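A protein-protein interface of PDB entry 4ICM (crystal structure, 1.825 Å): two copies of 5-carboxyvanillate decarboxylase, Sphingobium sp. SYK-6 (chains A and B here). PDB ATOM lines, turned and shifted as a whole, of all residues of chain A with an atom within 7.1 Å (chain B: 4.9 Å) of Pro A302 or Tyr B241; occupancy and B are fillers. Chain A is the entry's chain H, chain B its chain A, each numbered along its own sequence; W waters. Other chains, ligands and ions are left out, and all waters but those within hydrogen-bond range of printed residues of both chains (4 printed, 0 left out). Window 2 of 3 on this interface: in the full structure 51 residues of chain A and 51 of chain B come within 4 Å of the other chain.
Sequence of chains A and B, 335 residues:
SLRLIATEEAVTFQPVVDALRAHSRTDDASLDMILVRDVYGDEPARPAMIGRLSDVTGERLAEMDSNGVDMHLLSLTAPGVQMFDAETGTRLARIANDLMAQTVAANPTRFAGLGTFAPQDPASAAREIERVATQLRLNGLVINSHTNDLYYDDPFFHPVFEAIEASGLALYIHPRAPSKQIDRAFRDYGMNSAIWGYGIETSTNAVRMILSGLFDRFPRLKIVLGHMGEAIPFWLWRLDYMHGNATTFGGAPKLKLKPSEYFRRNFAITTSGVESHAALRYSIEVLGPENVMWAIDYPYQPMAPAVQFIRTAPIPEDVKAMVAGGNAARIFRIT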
ATOM      1  N   ARG A  52      13.056  -4.383  -5.096  1.00  0.00           N
ATOM      2  CA  ARG A  52      12.523  -3.998  -3.789  1.00  0.00           C
ATOM      3  C   ARG A  52      11.217  -4.733  -3.500  1.00  0.00           C
ATOM      4  O   ARG A  52      10.952  -5.129  -2.368  1.00  0.00           O
ATOM      5  CB  ARG A  52      12.354  -2.478  -3.680  1.00  0.00           C
ATOM      6  CG  ARG A  52      13.667  -1.721  -3.831  1.00  0.00           C
ATOM      7  CD  ARG A  52      13.827  -0.553  -2.845  1.00  0.00           C
ATOM      8  NE  ARG A  52      12.712   0.377  -2.890  1.00  0.00           N
ATOM      9  CZ  ARG A  52      12.045   0.786  -1.815  1.00  0.00           C
ATOM     10  NH1 ARG A  52      12.389   0.357  -0.604  1.00  0.00           N
ATOM     11  NH2 ARG A  52      11.035   1.630  -1.954  1.00  0.00           N
ATOM     12  N   GLU A  63      14.720  -2.853   7.491  1.00  0.00           N
ATOM     13  CA  GLU A  63      13.916  -1.654   7.708  1.00  0.00           C
ATOM     14  C   GLU A  63      12.848  -1.887   8.783  1.00  0.00           C
ATOM     15  O   GLU A  63      12.561  -1.003   9.586  1.00  0.00           O
ATOM     16  CB  GLU A  63      13.249  -1.240   6.394  1.00  0.00           C
ATOM     17  CG  GLU A  63      14.130  -0.445   5.474  1.00  0.00           C
ATOM     18  CD  GLU A  63      14.175   1.008   5.877  1.00  0.00           C
ATOM     19  OE1 GLU A  63      13.082   1.604   6.021  1.00  0.00           O
ATOM     20  OE2 GLU A  63      15.292   1.544   6.056  1.00  0.00           O
ATOM     21  N   ASN A  67      12.882   0.131  12.470  1.00  0.00           N
ATOM     22  CA  ASN A  67      11.740   0.951  12.822  1.00  0.00           C
ATOM     23  C   ASN A  67      10.820   0.304  13.853  1.00  0.00           C
ATOM     24  O   ASN A  67       9.792   0.873  14.222  1.00  0.00           O
ATOM     25  CB  ASN A  67      10.970   1.312  11.559  1.00  0.00           C
ATOM     26  CG  ASN A  67      11.750   2.242  10.660  1.00  0.00           C
ATOM     27  OD1 ASN A  67      11.856   3.432  10.941  1.00  0.00           O
ATOM     28  ND2 ASN A  67      12.285   1.711   9.566  1.00  0.00           N
ATOM     29  N   ILE A 195      -1.763   9.124  -7.213  1.00  0.00           N
ATOM     30  CA  ILE A 195      -2.163  10.518  -6.972  1.00  0.00           C
ATOM     31  C   ILE A 195      -3.670  10.807  -7.150  1.00  0.00           C
ATOM     32  O   ILE A 195      -4.219  11.700  -6.498  1.00  0.00           O
ATOM     33  CB  ILE A 195      -1.307  11.517  -7.775  1.00  0.00           C
ATOM     34  CG1 ILE A 195      -1.339  12.894  -7.109  1.00  0.00           C
ATOM     35  CG2 ILE A 195      -1.745  11.579  -9.239  1.00  0.00           C
ATOM     36  CD1 ILE A 195      -0.438  13.914  -7.783  1.00  0.00           C
ATOM     37  N   GLY A 273      -0.643   5.212   2.844  1.00  0.00           N
ATOM     38  CA  GLY A 273      -0.547   6.406   2.022  1.00  0.00           C
ATOM     39  C   GLY A 273      -1.357   7.604   2.469  1.00  0.00           C
ATOM     40  O   GLY A 273      -1.466   8.587   1.725  1.00  0.00           O
ATOM     41  N   GLU A 275      -1.007   9.512   5.781  1.00  0.00           N
ATOM     42  CA  GLU A 275      -0.395   9.686   7.088  1.00  0.00           C
ATOM     43  C   GLU A 275      -0.820  11.028   7.672  1.00  0.00           C
ATOM     44  O   GLU A 275      -0.005  11.919   7.913  1.00  0.00           O
ATOM     45  CB  GLU A 275       1.135   9.516   6.994  1.00  0.00           C
ATOM     46  CG  GLU A 275       1.506   8.110   6.475  1.00  0.00           C
ATOM     47  CD  GLU A 275       2.963   7.964   6.067  1.00  0.00           C
ATOM     48  OE1 GLU A 275       3.772   8.873   6.353  1.00  0.00           O
ATOM     49  OE2 GLU A 275       3.280   6.937   5.436  1.00  0.00           O
ATOM     50  N   ILE A 296       1.739   0.496   5.787  1.00  0.00           N
ATOM     51  CA  ILE A 296       2.840   1.300   5.255  1.00  0.00           C
ATOM     52  C   ILE A 296       2.649   1.574   3.771  1.00  0.00           C
ATOM     53  O   ILE A 296       2.831   2.694   3.330  1.00  0.00           O
ATOM     54  CB  ILE A 296       4.189   0.589   5.446  1.00  0.00           C
ATOM     55  CG1 ILE A 296       4.433   0.324   6.935  1.00  0.00           C
ATOM     56  CG2 ILE A 296       5.343   1.433   4.863  1.00  0.00           C
ATOM     57  CD1 ILE A 296       5.617  -0.599   7.205  1.00  0.00           C
ATOM     58  N   ASP A 297       2.264   0.543   3.024  1.00  0.00           N
ATOM     59  CA  ASP A 297       2.261   0.563   1.556  1.00  0.00           C
ATOM     60  C   ASP A 297       3.695   0.497   1.011  1.00  0.00           C
ATOM     61  O   ASP A 297       4.018   1.116  -0.006  1.00  0.00           O
ATOM     62  CB  ASP A 297       1.518   1.787   1.003  1.00  0.00           C
ATOM     63  CG  ASP A 297       0.672   1.468  -0.205  1.00  0.00           C
ATOM     64  OD1 ASP A 297       0.903   0.405  -0.814  1.00  0.00           O
ATOM     65  OD2 ASP A 297      -0.216   2.295  -0.544  1.00  0.00           O
ATOM     66  N   TYR A 298       4.547  -0.250   1.715  1.00  0.00           N
ATOM     67  CA  TYR A 298       5.904  -0.547   1.275  1.00  0.00           C
ATOM     68  C   TYR A 298       5.828  -1.475   0.061  1.00  0.00           C
ATOM     69  O   TYR A 298       4.953  -2.344   0.006  1.00  0.00           O
ATOM     70  CB  TYR A 298       6.655  -1.236   2.426  1.00  0.00           C
ATOM     71  CG  TYR A 298       8.098  -1.541   2.112  1.00  0.00           C
ATOM     72  CD1 TYR A 298       9.083  -0.590   2.331  1.00  0.00           C
ATOM     73  CD2 TYR A 298       8.473  -2.779   1.598  1.00  0.00           C
ATOM     74  CE1 TYR A 298      10.410  -0.846   2.043  1.00  0.00           C
ATOM     75  CE2 TYR A 298       9.806  -3.050   1.298  1.00  0.00           C
ATOM     76  CZ  TYR A 298      10.769  -2.082   1.526  1.00  0.00           C
ATOM     77  OH  TYR A 298      12.099  -2.336   1.238  1.00  0.00           O
ATOM     78  N   PRO A 299       6.748  -1.318  -0.913  1.00  0.00           N
ATOM     79  CA  PRO A 299       7.885  -0.390  -1.001  1.00  0.00           C
ATOM     80  C   PRO A 299       7.577   0.946  -1.686  1.00  0.00           C
ATOM     81  O   PRO A 299       8.512   1.708  -1.973  1.00  0.00           O
ATOM     82  CB  PRO A 299       8.893  -1.175  -1.842  1.00  0.00           C
ATOM     83  CG  PRO A 299       8.021  -1.934  -2.789  1.00  0.00           C
ATOM     84  CD  PRO A 299       6.761  -2.290  -2.020  1.00  0.00           C
ATOM     85  N   TYR A 300       6.301   1.235  -1.929  1.00  0.00           N
ATOM     86  CA  TYR A 300       5.921   2.493  -2.577  1.00  0.00           C
ATOM     87  C   TYR A 300       5.963   3.677  -1.624  1.00  0.00           C
ATOM     88  O   TYR A 300       6.070   4.822  -2.066  1.00  0.00           O
ATOM     89  CB  TYR A 300       4.539   2.363  -3.225  1.00  0.00           C
ATOM     90  CG  TYR A 300       4.454   1.177  -4.153  1.00  0.00           C
ATOM     91  CD1 TYR A 300       4.925   1.257  -5.463  1.00  0.00           C
ATOM     92  CD2 TYR A 300       3.934  -0.036  -3.713  1.00  0.00           C
ATOM     93  CE1 TYR A 300       4.861   0.168  -6.310  1.00  0.00           C
ATOM     94  CE2 TYR A 300       3.871  -1.135  -4.556  1.00  0.00           C
ATOM     95  CZ  TYR A 300       4.334  -1.030  -5.853  1.00  0.00           C
ATOM     96  OH  TYR A 300       4.266  -2.131  -6.689  1.00  0.00           O
ATOM     97  N   GLN A 301       5.860   3.395  -0.322  1.00  0.00           N
ATOM     98  CA  GLN A 301       6.011   4.395   0.740  1.00  0.00           C
ATOM     99  C   GLN A 301       7.159   3.920   1.636  1.00  0.00           C
ATOM    100  O   GLN A 301       7.322   2.722   1.846  1.00  0.00           O
ATOM    101  CB  GLN A 301       4.749   4.468   1.606  1.00  0.00           C
ATOM    102  CG  GLN A 301       3.425   4.821   0.894  1.00  0.00           C
ATOM    103  CD  GLN A 301       3.108   6.295   0.902  1.00  0.00           C
ATOM    104  OE1 GLN A 301       3.656   7.069   1.692  1.00  0.00           O
ATOM    105  NE2 GLN A 301       2.210   6.700   0.021  1.00  0.00           N
ATOM    106  N   PRO A 302       7.949   4.850   2.180  1.00  0.00           N
ATOM    107  CA  PRO A 302       9.002   4.473   3.131  1.00  0.00           C
ATOM    108  C   PRO A 302       8.426   4.110   4.497  1.00  0.00           C
ATOM    109  O   PRO A 302       7.369   4.629   4.886  1.00  0.00           O
ATOM    110  CB  PRO A 302       9.836   5.748   3.237  1.00  0.00           C
ATOM    111  CG  PRO A 302       8.857   6.850   2.933  1.00  0.00           C
ATOM    112  CD  PRO A 302       7.970   6.291   1.869  1.00  0.00           C
ATOM    113  N   MET A 303       9.121   3.246   5.232  1.00  0.00           N
ATOM    114  CA  MET A 303       8.576   2.727   6.481  1.00  0.00           C
ATOM    115  C   MET A 303       8.615   3.746   7.617  1.00  0.00           C
ATOM    116  O   MET A 303       7.632   3.882   8.358  1.00  0.00           O
ATOM    117  CB  MET A 303       9.306   1.442   6.912  1.00  0.00           C
ATOM    118  CG  MET A 303       8.983   0.249   6.046  1.00  0.00           C
ATOM    119  SD  MET A 303       9.461  -1.292   6.851  1.00  0.00           S
ATOM    120  CE  MET A 303      10.010  -2.210   5.408  1.00  0.00           C
ATOM    121  N   ALA A 304       9.741   4.447   7.756  1.00  0.00           N
ATOM    122  CA  ALA A 304       9.933   5.348   8.910  1.00  0.00           C
ATOM    123  C   ALA A 304       8.791   6.356   9.144  1.00  0.00           C
ATOM    124  O   ALA A 304       8.278   6.455  10.270  1.00  0.00           O
ATOM    125  CB  ALA A 304      11.296   6.045   8.860  1.00  0.00           C
ATOM    126  N   PRO A 305       8.389   7.107   8.097  1.00  0.00           N
ATOM    127  CA  PRO A 305       7.323   8.088   8.332  1.00  0.00           C
ATOM    128  C   PRO A 305       5.987   7.411   8.632  1.00  0.00           C
ATOM    129  O   PRO A 305       5.221   7.914   9.443  1.00  0.00           O
ATOM    130  CB  PRO A 305       7.249   8.865   7.004  1.00  0.00           C
ATOM    131  CG  PRO A 305       8.548   8.616   6.325  1.00  0.00           C
ATOM    132  CD  PRO A 305       8.977   7.245   6.748  1.00  0.00           C
ATOM    133  N   ALA A 306       5.715   6.267   8.012  1.00  0.00           N
ATOM    134  CA  ALA A 306       4.472   5.549   8.318  1.00  0.00           C
ATOM    135  C   ALA A 306       4.443   5.105   9.780  1.00  0.00           C
ATOM    136  O   ALA A 306       3.416   5.213  10.454  1.00  0.00           O
ATOM    137  CB  ALA A 306       4.290   4.351   7.387  1.00  0.00           C
ATOM    138  N   VAL A 307       5.583   4.622  10.264  1.00  0.00           N
ATOM    139  CA  VAL A 307       5.709   4.197  11.656  1.00  0.00           C
ATOM    140  C   VAL A 307       5.528   5.370  12.619  1.00  0.00           C
ATOM    141  O   VAL A 307       4.736   5.300  13.557  1.00  0.00           O
ATOM    142  CB  VAL A 307       7.075   3.536  11.903  1.00  0.00           C
ATOM    143  CG1 VAL A 307       7.324   3.314  13.403  1.00  0.00           C
ATOM    144  CG2 VAL A 307       7.144   2.224  11.148  1.00  0.00           C
ATOM    145  N   TRP B 237      -3.294  14.938   1.887  1.00  0.00           N
ATOM    146  CA  TRP B 237      -1.966  14.412   2.219  1.00  0.00           C
ATOM    147  C   TRP B 237      -1.430  13.556   1.069  1.00  0.00           C
ATOM    148  O   TRP B 237      -0.270  13.697   0.654  1.00  0.00           O
ATOM    149  CB  TRP B 237      -1.980  13.623   3.539  1.00  0.00           C
ATOM    150  CG  TRP B 237      -0.586  13.334   4.070  1.00  0.00           C
ATOM    151  CD1 TRP B 237       0.123  14.088   4.962  1.00  0.00           C
ATOM    152  CD2 TRP B 237       0.256  12.236   3.718  1.00  0.00           C
ATOM    153  NE1 TRP B 237       1.353  13.524   5.191  1.00  0.00           N
ATOM    154  CE2 TRP B 237       1.459  12.380   4.446  1.00  0.00           C
ATOM    155  CE3 TRP B 237       0.113  11.137   2.860  1.00  0.00           C
ATOM    156  CZ2 TRP B 237       2.515  11.470   4.339  1.00  0.00           C
ATOM    157  CZ3 TRP B 237       1.170  10.226   2.756  1.00  0.00           C
ATOM    158  CH2 TRP B 237       2.352  10.404   3.491  1.00  0.00           C
ATOM    159  N   ARG B 238      -2.292  12.696   0.538  1.00  0.00           N
ATOM    160  CA  ARG B 238      -1.917  11.782  -0.539  1.00  0.00           C
ATOM    161  C   ARG B 238      -1.678  12.542  -1.840  1.00  0.00           C
ATOM    162  O   ARG B 238      -0.771  12.209  -2.596  1.00  0.00           O
ATOM    163  CB  ARG B 238      -2.998  10.709  -0.719  1.00  0.00           C
ATOM    164  CG  ARG B 238      -2.716   9.601  -1.757  1.00  0.00           C
ATOM    165  CD  ARG B 238      -3.536   8.365  -1.362  1.00  0.00           C
ATOM    166  NE  ARG B 238      -3.579   7.257  -2.322  1.00  0.00           N
ATOM    167  CZ  ARG B 238      -2.599   6.383  -2.557  1.00  0.00           C
ATOM    168  NH1 ARG B 238      -1.412   6.495  -1.950  1.00  0.00           N
ATOM    169  NH2 ARG B 238      -2.802   5.396  -3.436  1.00  0.00           N
ATOM    170  N   LEU B 239      -2.490  13.557  -2.116  1.00  0.00           N
ATOM    171  CA  LEU B 239      -2.228  14.426  -3.272  1.00  0.00           C
ATOM    172  C   LEU B 239      -0.817  15.013  -3.217  1.00  0.00           C
ATOM    173  O   LEU B 239      -0.074  14.952  -4.196  1.00  0.00           O
ATOM    174  CB  LEU B 239      -3.254  15.562  -3.360  1.00  0.00           C
ATOM    175  CG  LEU B 239      -4.653  15.172  -3.827  1.00  0.00           C
ATOM    176  CD1 LEU B 239      -5.626  16.304  -3.543  1.00  0.00           C
ATOM    177  CD2 LEU B 239      -4.618  14.881  -5.335  1.00  0.00           C
ATOM    178  N   ASP B 240      -0.449  15.570  -2.065  1.00  0.00           N
ATOM    179  CA  ASP B 240       0.890  16.119  -1.874  1.00  0.00           C
ATOM    180  C   ASP B 240       1.957  15.045  -1.956  1.00  0.00           C
ATOM    181  O   ASP B 240       2.979  15.231  -2.623  1.00  0.00           O
ATOM    182  CB  ASP B 240       1.025  16.785  -0.504  1.00  0.00           C
ATOM    183  CG  ASP B 240       0.324  18.127  -0.428  1.00  0.00           C
ATOM    184  OD1 ASP B 240      -0.145  18.628  -1.471  1.00  0.00           O
ATOM    185  OD2 ASP B 240       0.242  18.682   0.685  1.00  0.00           O
ATOM    186  N   TYR B 241       1.751  13.940  -1.241  1.00  0.00           N
ATOM    187  CA  TYR B 241       2.811  12.936  -1.182  1.00  0.00           C
ATOM    188  C   TYR B 241       3.158  12.387  -2.577  1.00  0.00           C
ATOM    189  O   TYR B 241       4.333  12.223  -2.930  1.00  0.00           O
ATOM    190  CB  TYR B 241       2.492  11.783  -0.222  1.00  0.00           C
ATOM    191  CG  TYR B 241       3.666  10.810  -0.180  1.00  0.00           C
ATOM    192  CD1 TYR B 241       4.737  11.031   0.681  1.00  0.00           C
ATOM    193  CD2 TYR B 241       3.733   9.725  -1.056  1.00  0.00           C
ATOM    194  CE1 TYR B 241       5.831  10.188   0.692  1.00  0.00           C
ATOM    195  CE2 TYR B 241       4.825   8.875  -1.060  1.00  0.00           C
ATOM    196  CZ  TYR B 241       5.865   9.112  -0.180  1.00  0.00           C
ATOM    197  OH  TYR B 241       6.948   8.284  -0.183  1.00  0.00           O
ATOM    198  N   MET B 242       2.132  12.079  -3.353  1.00  0.00           N
ATOM    199  CA  MET B 242       2.331  11.421  -4.633  1.00  0.00           C
ATOM    200  C   MET B 242       2.704  12.379  -5.756  1.00  0.00           C
ATOM    201  O   MET B 242       3.019  11.951  -6.863  1.00  0.00           O
ATOM    202  CB  MET B 242       1.080  10.606  -4.985  1.00  0.00           C
ATOM    203  CG  MET B 242       0.962   9.337  -4.137  1.00  0.00           C
ATOM    204  SD  MET B 242       2.359   8.265  -4.533  1.00  0.00           S
ATOM    205  CE  MET B 242       2.226   6.996  -3.276  1.00  0.00           C
ATOM    206  N   HIS B 243       2.698  13.678  -5.474  1.00  0.00           N
ATOM    207  CA  HIS B 243       2.970  14.647  -6.527  1.00  0.00           C
ATOM    208  C   HIS B 243       4.408  14.562  -7.056  1.00  0.00           C
ATOM    209  O   HIS B 243       4.658  14.839  -8.225  1.00  0.00           O
ATOM    210  CB  HIS B 243       2.637  16.059  -6.071  1.00  0.00           C
ATOM    211  CG  HIS B 243       2.698  17.061  -7.176  1.00  0.00           C
ATOM    212  ND1 HIS B 243       3.491  18.186  -7.118  1.00  0.00           N
ATOM    213  CD2 HIS B 243       2.091  17.087  -8.386  1.00  0.00           C
ATOM    214  CE1 HIS B 243       3.346  18.876  -8.237  1.00  0.00           C
ATOM    215  NE2 HIS B 243       2.513  18.226  -9.027  1.00  0.00           N
ATOM    216  N   GLY B 244       5.339  14.155  -6.203  1.00  0.00           N
ATOM    217  CA  GLY B 244       6.712  13.922  -6.630  1.00  0.00           C
ATOM    218  C   GLY B 244       6.842  12.868  -7.724  1.00  0.00           C
ATOM    219  O   GLY B 244       7.523  13.080  -8.735  1.00  0.00           O
HETATM  220  O   HOH W   1       0.670   4.742  -1.197  1.00  0.00           O
HETATM  221  O   HOH W   2       0.187   8.557  -0.537  1.00  0.00           O
HETATM  222  O   HOH W   3      -0.552   3.440  -3.762  1.00  0.00           O
HETATM  223  O   HOH W   4       7.708   6.904  -2.212  1.00  0.00           O
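Pro A299 touches none of the printed residues of chain B.
Printed residues of chain A within 4 Å of Trp B237: Gly A273 and Glu A275.
Of chain A, only Gln A301 and Pro A302 come within 4 Å of Tyr B241.
Of the printed residues of chain A, Met B242 touches Ile A195 and Gln A301.
The nearest printed residue of chain B that does not touch Pro A302 is Trp B237 (7.1 Å).
The nearest residue of chain A that does not touch Tyr B241 is Tyr A300 (4.04 Å).
Of the 18 printed residues of chain A, 5 touch a printed residue of chain B.
Hydrophobic or aromatic side chains of chain A that line the printed part of chain B: Ile A195 and Pro A302.
Of the 8 printed residues of chain B, 6 touch a printed residue of chain A.
Among the printed residues, 9 pairs touch across the chains.
Among the printed residues, no Asp or Glu carboxylate lies within 4 Å of a Lys or Arg side-chain nitrogen of the other chain.
The indole nitrogen of Trp B237 sits at hydrogen-bond distance from the backbone carbonyl oxygen of Glu A275.
Water W4 lies within hydrogen-bond range of the side-chain hydroxyl of Tyr B241 (2.6 Å) and the backbone carbonyl oxygen of Tyr A300 (2.7 Å).
Water W1 lies within hydrogen-bond range of the side-chain carboxylate (OD2) of Asp A297 (2.7 Å), the side-chain amide nitrogen (NE2) of Gln A301 (2.8 Å) and the guanidinium group (NH1) of Arg B238 (2.8 Å).
Water W2 lies within hydrogen-bond range of the backbone carbonyl oxygen of Gly A273 (2.8 Å), the side-chain amide nitrogen of Gln A301 (2.8 Å) and the guanidinium group of Arg B238 (3.0 Å).
Water W3 bridges NH2 of Arg B238 and OD2 of Asp A297.
Among the printed residues, merely in contact across the chains: Ile A195 with Leu B239 (3.4 Å), Ile A195 with Met B242 (3.8 Å), Ile A195 with His B243 (3.7 Å), Gly A273 with Trp B237 (3.2 Å), Gly A273 with Arg B238 (3.6 Å), Gln A301 with Tyr B241 (3.5 Å), Gln A301 with Met B242 (3.3 Å) and Pro A302 with Tyr B241 (3.0 Å).
No position is printed for both chains.
Of the 9 pairs that touch across the chains among the printed residues, none has its exchanged pair printed and touching as well.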
